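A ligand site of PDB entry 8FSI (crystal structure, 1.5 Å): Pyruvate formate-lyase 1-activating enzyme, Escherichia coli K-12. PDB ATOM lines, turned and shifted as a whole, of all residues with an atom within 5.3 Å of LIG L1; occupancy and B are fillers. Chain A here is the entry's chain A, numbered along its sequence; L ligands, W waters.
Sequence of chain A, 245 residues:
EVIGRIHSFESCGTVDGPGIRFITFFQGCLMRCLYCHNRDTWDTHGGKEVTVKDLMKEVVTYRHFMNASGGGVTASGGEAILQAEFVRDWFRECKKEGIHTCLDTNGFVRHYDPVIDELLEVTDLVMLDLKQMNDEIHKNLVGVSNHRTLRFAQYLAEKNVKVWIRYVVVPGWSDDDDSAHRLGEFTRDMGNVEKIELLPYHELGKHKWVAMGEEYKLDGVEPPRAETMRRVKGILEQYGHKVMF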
ATOM      1  N   CYS A  29       4.016 -32.600 -17.890  1.00  0.00           N
ATOM      2  CA  CYS A  29       5.356 -33.106 -17.634  1.00  0.00           C
ATOM      3  C   CYS A  29       5.317 -34.605 -17.816  1.00  0.00           C
ATOM      4  O   CYS A  29       4.325 -35.244 -17.431  1.00  0.00           O
ATOM      5  CB  CYS A  29       5.798 -32.775 -16.218  1.00  0.00           C
ATOM      6  SG  CYS A  29       7.560 -33.201 -15.986  1.00  0.00           S
ATOM      7  N   TYR A  35       9.536 -36.260  -5.527  1.00  0.00           N
ATOM      8  CA  TYR A  35       9.489 -35.052  -4.732  1.00  0.00           C
ATOM      9  C   TYR A  35       8.700 -33.919  -5.359  1.00  0.00           C
ATOM     10  O   TYR A  35       8.567 -32.892  -4.713  1.00  0.00           O
ATOM     11  CB  TYR A  35      10.924 -34.576  -4.447  1.00  0.00           C
ATOM     12  CG  TYR A  35      11.883 -34.404  -5.616  1.00  0.00           C
ATOM     13  CD1 TYR A  35      11.762 -33.376  -6.512  1.00  0.00           C
ATOM     14  CD2 TYR A  35      12.944 -35.277  -5.782  1.00  0.00           C
ATOM     15  CE1 TYR A  35      12.681 -33.217  -7.547  1.00  0.00           C
ATOM     16  CE2 TYR A  35      13.870 -35.132  -6.788  1.00  0.00           C
ATOM     17  CZ  TYR A  35      13.736 -34.101  -7.643  1.00  0.00           C
ATOM     18  OH  TYR A  35      14.655 -33.883  -8.651  1.00  0.00           O
ATOM     19  N   CYS A  36       8.188 -34.069  -6.563  1.00  0.00           N
ATOM     20  CA  CYS A  36       7.684 -32.918  -7.305  1.00  0.00           C
ATOM     21  C   CYS A  36       6.799 -32.045  -6.443  1.00  0.00           C
ATOM     22  O   CYS A  36       5.757 -32.479  -5.945  1.00  0.00           O
ATOM     23  CB  CYS A  36       6.869 -33.386  -8.487  1.00  0.00           C
ATOM     24  SG  CYS A  36       6.388 -31.979  -9.553  1.00  0.00           S
ATOM     25  N   HIS A  37       7.145 -30.776  -6.324  1.00  0.00           N
ATOM     26  CA  HIS A  37       6.336 -29.846  -5.560  1.00  0.00           C
ATOM     27  C   HIS A  37       5.213 -29.209  -6.368  1.00  0.00           C
ATOM     28  O   HIS A  37       4.450 -28.420  -5.781  1.00  0.00           O
ATOM     29  CB  HIS A  37       7.183 -28.789  -4.858  1.00  0.00           C
ATOM     30  CG  HIS A  37       7.955 -27.880  -5.736  1.00  0.00           C
ATOM     31  ND1 HIS A  37       9.088 -27.232  -5.301  1.00  0.00           N
ATOM     32  CD2 HIS A  37       7.734 -27.452  -6.998  1.00  0.00           C
ATOM     33  CE1 HIS A  37       9.545 -26.454  -6.262  1.00  0.00           C
ATOM     34  NE2 HIS A  37       8.747 -26.564  -7.311  1.00  0.00           N
ATOM     35  N   ASN A  38       5.070 -29.593  -7.640  1.00  0.00           N
ATOM     36  CA  ASN A  38       4.022 -29.129  -8.539  1.00  0.00           C
ATOM     37  C   ASN A  38       3.271 -30.311  -9.168  1.00  0.00           C
ATOM     38  O   ASN A  38       3.155 -30.411 -10.390  1.00  0.00           O
ATOM     39  CB  ASN A  38       4.570 -28.234  -9.661  1.00  0.00           C
ATOM     40  CG  ASN A  38       5.071 -26.901  -9.168  1.00  0.00           C
ATOM     41  OD1 ASN A  38       4.727 -26.461  -8.092  1.00  0.00           O
ATOM     42  ND2 ASN A  38       5.833 -26.206 -10.013  1.00  0.00           N
ATOM     43  N   SER A  76       8.732 -22.224 -16.970  1.00  0.00           N
ATOM     44  CA  SER A  76       8.871 -23.304 -16.008  1.00  0.00           C
ATOM     45  C   SER A  76       7.613 -24.162 -16.139  1.00  0.00           C
ATOM     46  O   SER A  76       6.956 -24.218 -17.176  1.00  0.00           O
ATOM     47  CB  SER A  76       9.048 -22.752 -14.597  1.00  0.00           C
ATOM     48  OG  SER A  76       9.320 -23.770 -13.630  1.00  0.00           O
ATOM     49  N   GLY A  77       7.243 -24.875 -15.084  1.00  0.00           N
ATOM     50  CA  GLY A  77       6.122 -25.792 -15.129  1.00  0.00           C
ATOM     51  C   GLY A  77       6.154 -26.800 -14.011  1.00  0.00           C
ATOM     52  O   GLY A  77       6.537 -26.434 -12.897  1.00  0.00           O
ATOM     53  N   GLY A  78       5.718 -28.033 -14.241  1.00  0.00           N
ATOM     54  CA  GLY A  78       5.576 -28.647 -15.550  1.00  0.00           C
ATOM     55  C   GLY A  78       6.873 -28.616 -16.301  1.00  0.00           C
ATOM     56  O   GLY A  78       7.896 -28.054 -15.819  1.00  0.00           O
ATOM     57  N   GLU A  79       6.858 -29.123 -17.535  1.00  0.00           N
ATOM     58  CA  GLU A  79       8.011 -29.140 -18.406  1.00  0.00           C
ATOM     59  C   GLU A  79       7.789 -28.330 -19.670  1.00  0.00           C
ATOM     60  O   GLU A  79       7.095 -28.780 -20.599  1.00  0.00           O
ATOM     61  CB  GLU A  79       8.461 -30.530 -18.794  1.00  0.00           C
ATOM     62  CG  GLU A  79       9.690 -30.517 -19.634  1.00  0.00           C
ATOM     63  CD  GLU A  79      10.780 -29.571 -19.109  1.00  0.00           C
ATOM     64  OE1 GLU A  79      11.107 -29.654 -17.901  1.00  0.00           O
ATOM     65  OE2 GLU A  79      11.247 -28.685 -19.881  1.00  0.00           O
ATOM     66  N   ASP A 104      13.524 -23.103 -17.626  1.00  0.00           N
ATOM     67  CA  ASP A 104      13.689 -23.975 -16.448  1.00  0.00           C
ATOM     68  C   ASP A 104      13.210 -25.368 -16.796  1.00  0.00           C
ATOM     69  O   ASP A 104      12.016 -25.618 -16.827  1.00  0.00           O
ATOM     70  CB  ASP A 104      12.859 -23.388 -15.314  1.00  0.00           C
ATOM     71  CG  ASP A 104      12.856 -24.207 -14.039  1.00  0.00           C
ATOM     72  OD1 ASP A 104      13.804 -24.980 -13.845  1.00  0.00           O
ATOM     73  OD2 ASP A 104      11.943 -23.997 -13.197  1.00  0.00           O
ATOM     74  N   THR A 105      14.138 -26.275 -17.053  1.00  0.00           N
ATOM     75  CA  THR A 105      13.846 -27.527 -17.743  1.00  0.00           C
ATOM     76  C   THR A 105      14.477 -28.746 -17.121  1.00  0.00           C
ATOM     77  O   THR A 105      15.553 -28.695 -16.525  1.00  0.00           O
ATOM     78  CB  THR A 105      14.248 -27.439 -19.241  1.00  0.00           C
ATOM     79  OG1 THR A 105      13.924 -28.607 -19.999  1.00  0.00           O
ATOM     80  CG2 THR A 105      15.752 -27.228 -19.428  1.00  0.00           C
ATOM     81  N   ASN A 106      13.763 -29.870 -17.297  1.00  0.00           N
ATOM     82  CA  ASN A 106      14.280 -31.188 -16.976  1.00  0.00           C
ATOM     83  C   ASN A 106      15.097 -31.788 -18.124  1.00  0.00           C
ATOM     84  O   ASN A 106      15.646 -32.870 -17.977  1.00  0.00           O
ATOM     85  CB  ASN A 106      13.140 -32.145 -16.618  1.00  0.00           C
ATOM     86  CG  ASN A 106      12.161 -32.439 -17.770  1.00  0.00           C
ATOM     87  OD1 ASN A 106      12.465 -32.234 -18.943  1.00  0.00           O
ATOM     88  ND2 ASN A 106      10.985 -32.980 -17.417  1.00  0.00           N
ATOM     89  N   MET A 127      18.238 -23.198 -17.031  1.00  0.00           N
ATOM     90  CA  MET A 127      18.417 -23.842 -15.730  1.00  0.00           C
ATOM     91  C   MET A 127      18.039 -25.300 -15.895  1.00  0.00           C
ATOM     92  O   MET A 127      16.848 -25.643 -15.917  1.00  0.00           O
ATOM     93  CB  MET A 127      17.570 -23.152 -14.671  1.00  0.00           C
ATOM     94  CG  MET A 127      17.871 -21.680 -14.538  1.00  0.00           C
ATOM     95  SD  MET A 127      17.120 -20.901 -13.094  1.00  0.00           S
ATOM     96  CE  MET A 127      15.420 -21.271 -13.395  1.00  0.00           C
ATOM     97  N   ASP A 129      17.914 -29.133 -14.776  1.00  0.00           N
ATOM     98  CA  ASP A 129      18.022 -30.119 -13.689  1.00  0.00           C
ATOM     99  C   ASP A 129      18.777 -31.365 -14.151  1.00  0.00           C
ATOM    100  O   ASP A 129      18.485 -31.940 -15.206  1.00  0.00           O
ATOM    101  CB  ASP A 129      16.656 -30.617 -13.241  1.00  0.00           C
ATOM    102  CG  ASP A 129      16.140 -29.905 -12.031  1.00  0.00           C
ATOM    103  OD1 ASP A 129      16.209 -28.666 -11.975  1.00  0.00           O
ATOM    104  OD2 ASP A 129      15.661 -30.579 -11.088  1.00  0.00           O
ATOM    105  N   LYS A 131      19.031 -34.599 -12.200  1.00  0.00           N
ATOM    106  CA  LYS A 131      18.382 -35.063 -10.973  1.00  0.00           C
ATOM    107  C   LYS A 131      19.127 -36.202 -10.305  1.00  0.00           C
ATOM    108  O   LYS A 131      18.989 -36.379  -9.096  1.00  0.00           O
ATOM    109  CB  LYS A 131      16.940 -35.459 -11.239  1.00  0.00           C
ATOM    110  CG  LYS A 131      16.098 -34.257 -11.758  1.00  0.00           C
ATOM    111  CD  LYS A 131      14.710 -34.664 -12.134  1.00  0.00           C
ATOM    112  CE  LYS A 131      13.948 -33.493 -12.733  1.00  0.00           C
ATOM    113  NZ  LYS A 131      13.508 -32.517 -11.661  1.00  0.00           N
ATOM    114  N   ARG A 166      21.082 -27.485 -11.922  1.00  0.00           N
ATOM    115  CA  ARG A 166      20.366 -27.577 -10.651  1.00  0.00           C
ATOM    116  C   ARG A 166      20.273 -29.019 -10.194  1.00  0.00           C
ATOM    117  O   ARG A 166      19.880 -29.894 -10.955  1.00  0.00           O
ATOM    118  CB  ARG A 166      18.967 -26.987 -10.842  1.00  0.00           C
ATOM    119  CG  ARG A 166      18.971 -25.498 -11.192  1.00  0.00           C
ATOM    120  CD  ARG A 166      18.664 -24.803  -9.936  1.00  0.00           C
ATOM    121  NE  ARG A 166      18.726 -23.356  -9.991  1.00  0.00           N
ATOM    122  CZ  ARG A 166      17.678 -22.552  -9.929  1.00  0.00           C
ATOM    123  NH1 ARG A 166      16.454 -22.973 -10.170  1.00  0.00           N
ATOM    124  NH2 ARG A 166      17.872 -21.281  -9.620  1.00  0.00           N
ATOM    125  N   VAL A 168      18.673 -31.175  -7.044  1.00  0.00           N
ATOM    126  CA  VAL A 168      17.855 -31.286  -5.828  1.00  0.00           C
ATOM    127  C   VAL A 168      18.443 -32.385  -4.963  1.00  0.00           C
ATOM    128  O   VAL A 168      18.499 -33.545  -5.377  1.00  0.00           O
ATOM    129  CB  VAL A 168      16.395 -31.578  -6.168  1.00  0.00           C
ATOM    130  CG1 VAL A 168      15.583 -31.704  -4.923  1.00  0.00           C
ATOM    131  CG2 VAL A 168      15.787 -30.483  -7.055  1.00  0.00           C
ATOM    132  N   LEU A 199      19.694 -27.425  -4.655  1.00  0.00           N
ATOM    133  CA  LEU A 199      18.384 -27.083  -4.112  1.00  0.00           C
ATOM    134  C   LEU A 199      18.083 -28.081  -3.017  1.00  0.00           C
ATOM    135  O   LEU A 199      17.929 -29.286  -3.284  1.00  0.00           O
ATOM    136  CB  LEU A 199      17.329 -27.160  -5.188  1.00  0.00           C
ATOM    137  CG  LEU A 199      17.424 -26.191  -6.342  1.00  0.00           C
ATOM    138  CD1 LEU A 199      16.342 -26.456  -7.365  1.00  0.00           C
ATOM    139  CD2 LEU A 199      17.409 -24.785  -5.855  1.00  0.00           C
ATOM    140  N   PRO A 200      17.999 -27.670  -1.771  1.00  0.00           N
ATOM    141  CA  PRO A 200      17.624 -28.641  -0.738  1.00  0.00           C
ATOM    142  C   PRO A 200      16.201 -29.132  -0.922  1.00  0.00           C
ATOM    143  O   PRO A 200      15.289 -28.337  -1.144  1.00  0.00           O
ATOM    144  CB  PRO A 200      17.759 -27.853   0.552  1.00  0.00           C
ATOM    145  CG  PRO A 200      17.502 -26.426   0.127  1.00  0.00           C
ATOM    146  CD  PRO A 200      18.129 -26.298  -1.255  1.00  0.00           C
ATOM    147  N   TYR A 201      16.006 -30.438  -0.764  1.00  0.00           N
ATOM    148  CA  TYR A 201      14.654 -30.989  -0.752  1.00  0.00           C
ATOM    149  C   TYR A 201      13.786 -30.295   0.306  1.00  0.00           C
ATOM    150  O   TYR A 201      14.219 -30.104   1.435  1.00  0.00           O
ATOM    151  CB  TYR A 201      14.682 -32.485  -0.457  1.00  0.00           C
ATOM    152  CG  TYR A 201      13.329 -33.052  -0.126  1.00  0.00           C
ATOM    153  CD1 TYR A 201      12.381 -33.248  -1.138  1.00  0.00           C
ATOM    154  CD2 TYR A 201      12.956 -33.379   1.167  1.00  0.00           C
ATOM    155  CE1 TYR A 201      11.140 -33.771  -0.838  1.00  0.00           C
ATOM    156  CE2 TYR A 201      11.711 -33.873   1.451  1.00  0.00           C
ATOM    157  CZ  TYR A 201      10.788 -34.045   0.440  1.00  0.00           C
ATOM    158  OH  TYR A 201       9.527 -34.557   0.760  1.00  0.00           O
ATOM    159  N   HIS A 202      12.556 -29.955  -0.082  1.00  0.00           N
ATOM    160  CA  HIS A 202      11.535 -29.480   0.833  1.00  0.00           C
ATOM    161  C   HIS A 202      10.253 -30.271   0.607  1.00  0.00           C
ATOM    162  O   HIS A 202       9.974 -30.734  -0.493  1.00  0.00           O
ATOM    163  CB  HIS A 202      11.256 -27.972   0.703  1.00  0.00           C
ATOM    164  CG  HIS A 202      10.974 -27.527  -0.696  1.00  0.00           C
ATOM    165  ND1 HIS A 202      11.796 -26.682  -1.386  1.00  0.00           N
ATOM    166  CD2 HIS A 202       9.963 -27.853  -1.538  1.00  0.00           C
ATOM    167  CE1 HIS A 202      11.315 -26.500  -2.604  1.00  0.00           C
ATOM    168  NE2 HIS A 202      10.205 -27.205  -2.711  1.00  0.00           N
ATOM    169  N   GLU A 203       9.424 -30.375   1.659  1.00  0.00           N
ATOM    170  CA  GLU A 203       8.196 -31.165   1.584  1.00  0.00           C
ATOM    171  C   GLU A 203       7.015 -30.384   1.010  1.00  0.00           C
ATOM    172  O   GLU A 203       5.953 -30.978   0.782  1.00  0.00           O
ATOM    173  CB  GLU A 203       7.812 -31.747   2.968  1.00  0.00           C
ATOM    174  CG  GLU A 203       6.596 -32.691   2.905  1.00  0.00           C
ATOM    175  CD  GLU A 203       6.304 -33.399   4.233  1.00  0.00           C
ATOM    176  OE1 GLU A 203       6.019 -32.712   5.235  1.00  0.00           O
ATOM    177  OE2 GLU A 203       6.370 -34.654   4.262  1.00  0.00           O
ATOM    178  N   LEU A 204       7.175 -29.081   0.743  1.00  0.00           N
ATOM    179  CA  LEU A 204       6.099 -28.283   0.167  1.00  0.00           C
ATOM    180  C   LEU A 204       5.493 -28.955  -1.063  1.00  0.00           C
ATOM    181  O   LEU A 204       6.201 -29.558  -1.877  1.00  0.00           O
ATOM    182  CB  LEU A 204       6.655 -26.926  -0.294  1.00  0.00           C
ATOM    183  CG  LEU A 204       7.532 -26.128   0.670  1.00  0.00           C
ATOM    184  CD1 LEU A 204       7.939 -24.819  -0.023  1.00  0.00           C
ATOM    185  CD2 LEU A 204       6.816 -25.874   1.974  1.00  0.00           C
ATOM    186  N   TYR A 216       2.001 -39.695  -1.368  1.00  0.00           N
ATOM    187  CA  TYR A 216       3.315 -39.088  -1.418  1.00  0.00           C
ATOM    188  C   TYR A 216       4.337 -40.085  -0.889  1.00  0.00           C
ATOM    189  O   TYR A 216       4.222 -40.548   0.250  1.00  0.00           O
ATOM    190  CB  TYR A 216       3.266 -37.821  -0.582  1.00  0.00           C
ATOM    191  CG  TYR A 216       4.499 -36.971  -0.756  1.00  0.00           C
ATOM    192  CD1 TYR A 216       4.807 -36.422  -1.980  1.00  0.00           C
ATOM    193  CD2 TYR A 216       5.360 -36.736   0.300  1.00  0.00           C
ATOM    194  CE1 TYR A 216       5.921 -35.665  -2.158  1.00  0.00           C
ATOM    195  CE2 TYR A 216       6.484 -35.974   0.144  1.00  0.00           C
ATOM    196  CZ  TYR A 216       6.750 -35.440  -1.103  1.00  0.00           C
ATOM    197  OH  TYR A 216       7.864 -34.683  -1.280  1.00  0.00           O
HETATM  198  N1  LIG L   1      10.187 -29.568 -14.698  1.00  0.00           N
HETATM  199  C1  LIG L   1      11.332 -28.668 -14.594  1.00  0.00           C
HETATM  200  C2  LIG L   1      12.336 -29.318 -13.699  1.00  0.00           C
HETATM  201  O1  LIG L   1      12.044 -30.259 -12.953  1.00  0.00           O
HETATM  202  O2  LIG L   1      13.483 -28.838 -13.712  1.00  0.00           O
HETATM  203  C3  LIG L   1      10.864 -27.287 -14.093  1.00  0.00           C
HETATM  204  C4  LIG L   1       9.774 -27.257 -13.028  1.00  0.00           C
HETATM  205  S1  LIG L   1      10.335 -27.836 -11.414  1.00  0.00           S
HETATM  206  C5  LIG L   1       8.798 -27.769 -10.429  1.00  0.00           C
HETATM  207  C6  LIG L   1      11.296 -26.405 -10.823  1.00  0.00           C
HETATM  208  C7  LIG L   1      12.415 -26.802  -9.886  1.00  0.00           C
HETATM  209  O3  LIG L   1      11.876 -27.265  -8.619  1.00  0.00           O
HETATM  210  C8  LIG L   1      13.317 -27.967 -10.336  1.00  0.00           C
HETATM  211  O4  LIG L   1      14.701 -27.619 -10.114  1.00  0.00           O
HETATM  212  C9  LIG L   1      12.864 -29.150  -9.520  1.00  0.00           C
HETATM  213  O5  LIG L   1      13.745 -30.207  -9.400  1.00  0.00           O
HETATM  214  C10 LIG L   1      12.613 -28.406  -8.192  1.00  0.00           C
HETATM  215  N2  LIG L   1      11.839 -29.125  -7.206  1.00  0.00           N
HETATM  216  C11 LIG L   1      10.720 -29.817  -7.484  1.00  0.00           C
HETATM  217  N3  LIG L   1      10.220 -30.390  -6.368  1.00  0.00           N
HETATM  218  C12 LIG L   1      11.092 -30.042  -5.328  1.00  0.00           C
HETATM  219  C13 LIG L   1      11.142 -30.316  -3.959  1.00  0.00           C
HETATM  220  N4  LIG L   1      10.232 -31.060  -3.361  1.00  0.00           N
HETATM  221  N5  LIG L   1      12.189 -29.783  -3.263  1.00  0.00           N
HETATM  222  C14 LIG L   1      13.136 -28.995  -3.824  1.00  0.00           C
HETATM  223  N6  LIG L   1      13.121 -28.692  -5.185  1.00  0.00           N
HETATM  224  C15 LIG L   1      12.108 -29.259  -5.865  1.00  0.00           C
HETATM  225 FE1  LG2 L   2       9.973 -33.573 -11.949  1.00  0.00          FE
HETATM  226 FE2  LG2 L   2       9.993 -30.948 -12.922  1.00  0.00          FE
HETATM  227 FE3  LG2 L   2       7.895 -32.032 -11.255  1.00  0.00          FE
HETATM  228 FE4  LG2 L   2       8.158 -32.799 -13.814  1.00  0.00          FE
HETATM  229  S1  LG2 L   2       7.598 -30.721 -13.039  1.00  0.00           S
HETATM  230  S2  LG2 L   2       7.795 -34.185 -12.125  1.00  0.00           S
HETATM  231  S3  LG2 L   2      10.462 -32.892 -14.024  1.00  0.00           S
HETATM  232  S4  LG2 L   2      10.103 -31.642 -10.682  1.00  0.00           S
HETATM  233  O   HOH W   1      11.533 -23.955  -7.914  1.00  0.00           O
HETATM  234  O   HOH W   2      13.532 -25.840  -5.076  1.00  0.00           O
HETATM  235  O   HOH W   3      15.473 -25.361 -11.544  1.00  0.00           O
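The side-chain carboxylate (OD2) of Asp 129 is in hydrogen-bond range of an oxygen (O5) of LIG L1, 2.6 Å away. N4 of LIG L1 lies within hydrogen-bond range of O of Tyr 35 (2.8 Å). The backbone NH (N) of His 202 is in hydrogen-bond range of a nitrogen (N5) of LIG L1, 3.2 Å away. The backbone carbonyl oxygen (O) of His 202 is in hydrogen-bond range of a nitrogen (N4) of LIG L1 (2.9 Å). A nitrogen (N5) of LIG L1 sits at hydrogen-bond distance from a ring nitrogen (NE2) of His 202, at 3.3 Å. O of Gly 78 sits close to N1 of LIG L1. O5 of LIG L1 is in hydrogen-bond range of NZ of Lys 131, at 3.2 Å. N of His 37 is in hydrogen-bond range of N3 of LIG L1, at 3.1 Å. NE2 of His 37 sits close to O3 of LIG L1 (3.5 Å). N1 of LIG L1 lies close to OE1 of Glu 79 (3.3 Å). N of Gly 78 sits close to S1 of LG2 L2. The side-chain amino group (NZ) of Lys 131 sits close to a sulfur (S4) of LG2 L2, 3.6 Å away. An iron atom (FE3) of LG2 L2 is bound by the side-chain sulfur (SG) of Cys 36 (2.3 Å). ND2 of Asn 106 lies close to S3 of LG2 L2 (3.4 Å). The side-chain sulfur (SG) of Cys 29 binds an iron atom (FE4) of LG2 L2.
FE2 of LG2 L2 is bound by O1 of LIG L1, at 2.2 Å.
O of Thr 105 is in hydrogen-bond range of N of Asp 129 (3.0 Å). The side-chain amino group (NZ) of Lys 131 lies close to the side-chain hydroxyl (OH) of Tyr 35 (3.5 Å). NE2 of His 202 is in hydrogen-bond range of ND1 of His 37. The side-chain amide nitrogen (ND2) of Asn 38 is in hydrogen-bond range of the backbone carbonyl oxygen (O) of Gly 77 (3.0 Å). SG of Cys 36 sits close to N of Asn 38, 3.3 Å away. The side-chain hydroxyl (OG) of Ser 76 sits at hydrogen-bond distance from the side-chain carboxylate (OD2) of Asp 104. The backbone carbonyl oxygen (O) of Met 127 sits at hydrogen-bond distance from the backbone NH (N) of Thr 105, at 3.0 Å. OH of Tyr 216 sits at hydrogen-bond distance from OH of Tyr 201, 2.6 Å away.
The backbone carbonyl oxygen (O) of Thr 105 sits close to an oxygen (O2) of LIG L1, 3.5 Å away. Merely in contact with LIG L1: Val 168 (3.1 Å), Gly 77 (3.3 Å), Asn 38 (3.4 Å), Asp 104 (3.4 Å), Leu 199 (3.4 Å), Pro 200 (3.5 Å), Ser 76 (3.6 Å), Cys 36 (3.7 Å), Tyr 201 (3.7 Å) and Asn 106 (3.7 Å). Hydrophobic or aromatic side chains that line LIG L1: Tyr 35, His 37, Val 168, Leu 199, Tyr 201 and His 202. 18 residues have an atom within 4 Å of LIG L1: Tyr 35, Cys 36, His 37, Asn 38, Ser 76, Gly 77, Gly 78, Glu 79, Asp 104, Thr 105, Asn 106, Asp 129, Lys 131, Val 168, Leu 199, Pro 200, Tyr 201 and His 202. The nearest printed residue that does not touch LIG L1 is Arg 166 (4.4 Å).
Water W3 lies within hydrogen-bond range of O4 of LIG L1 (2.8 Å), OD1 of Asp 104 (2.9 Å), NH1 of Arg 166 (2.9 Å) and OD1 of Asp 129 (3.4 Å).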
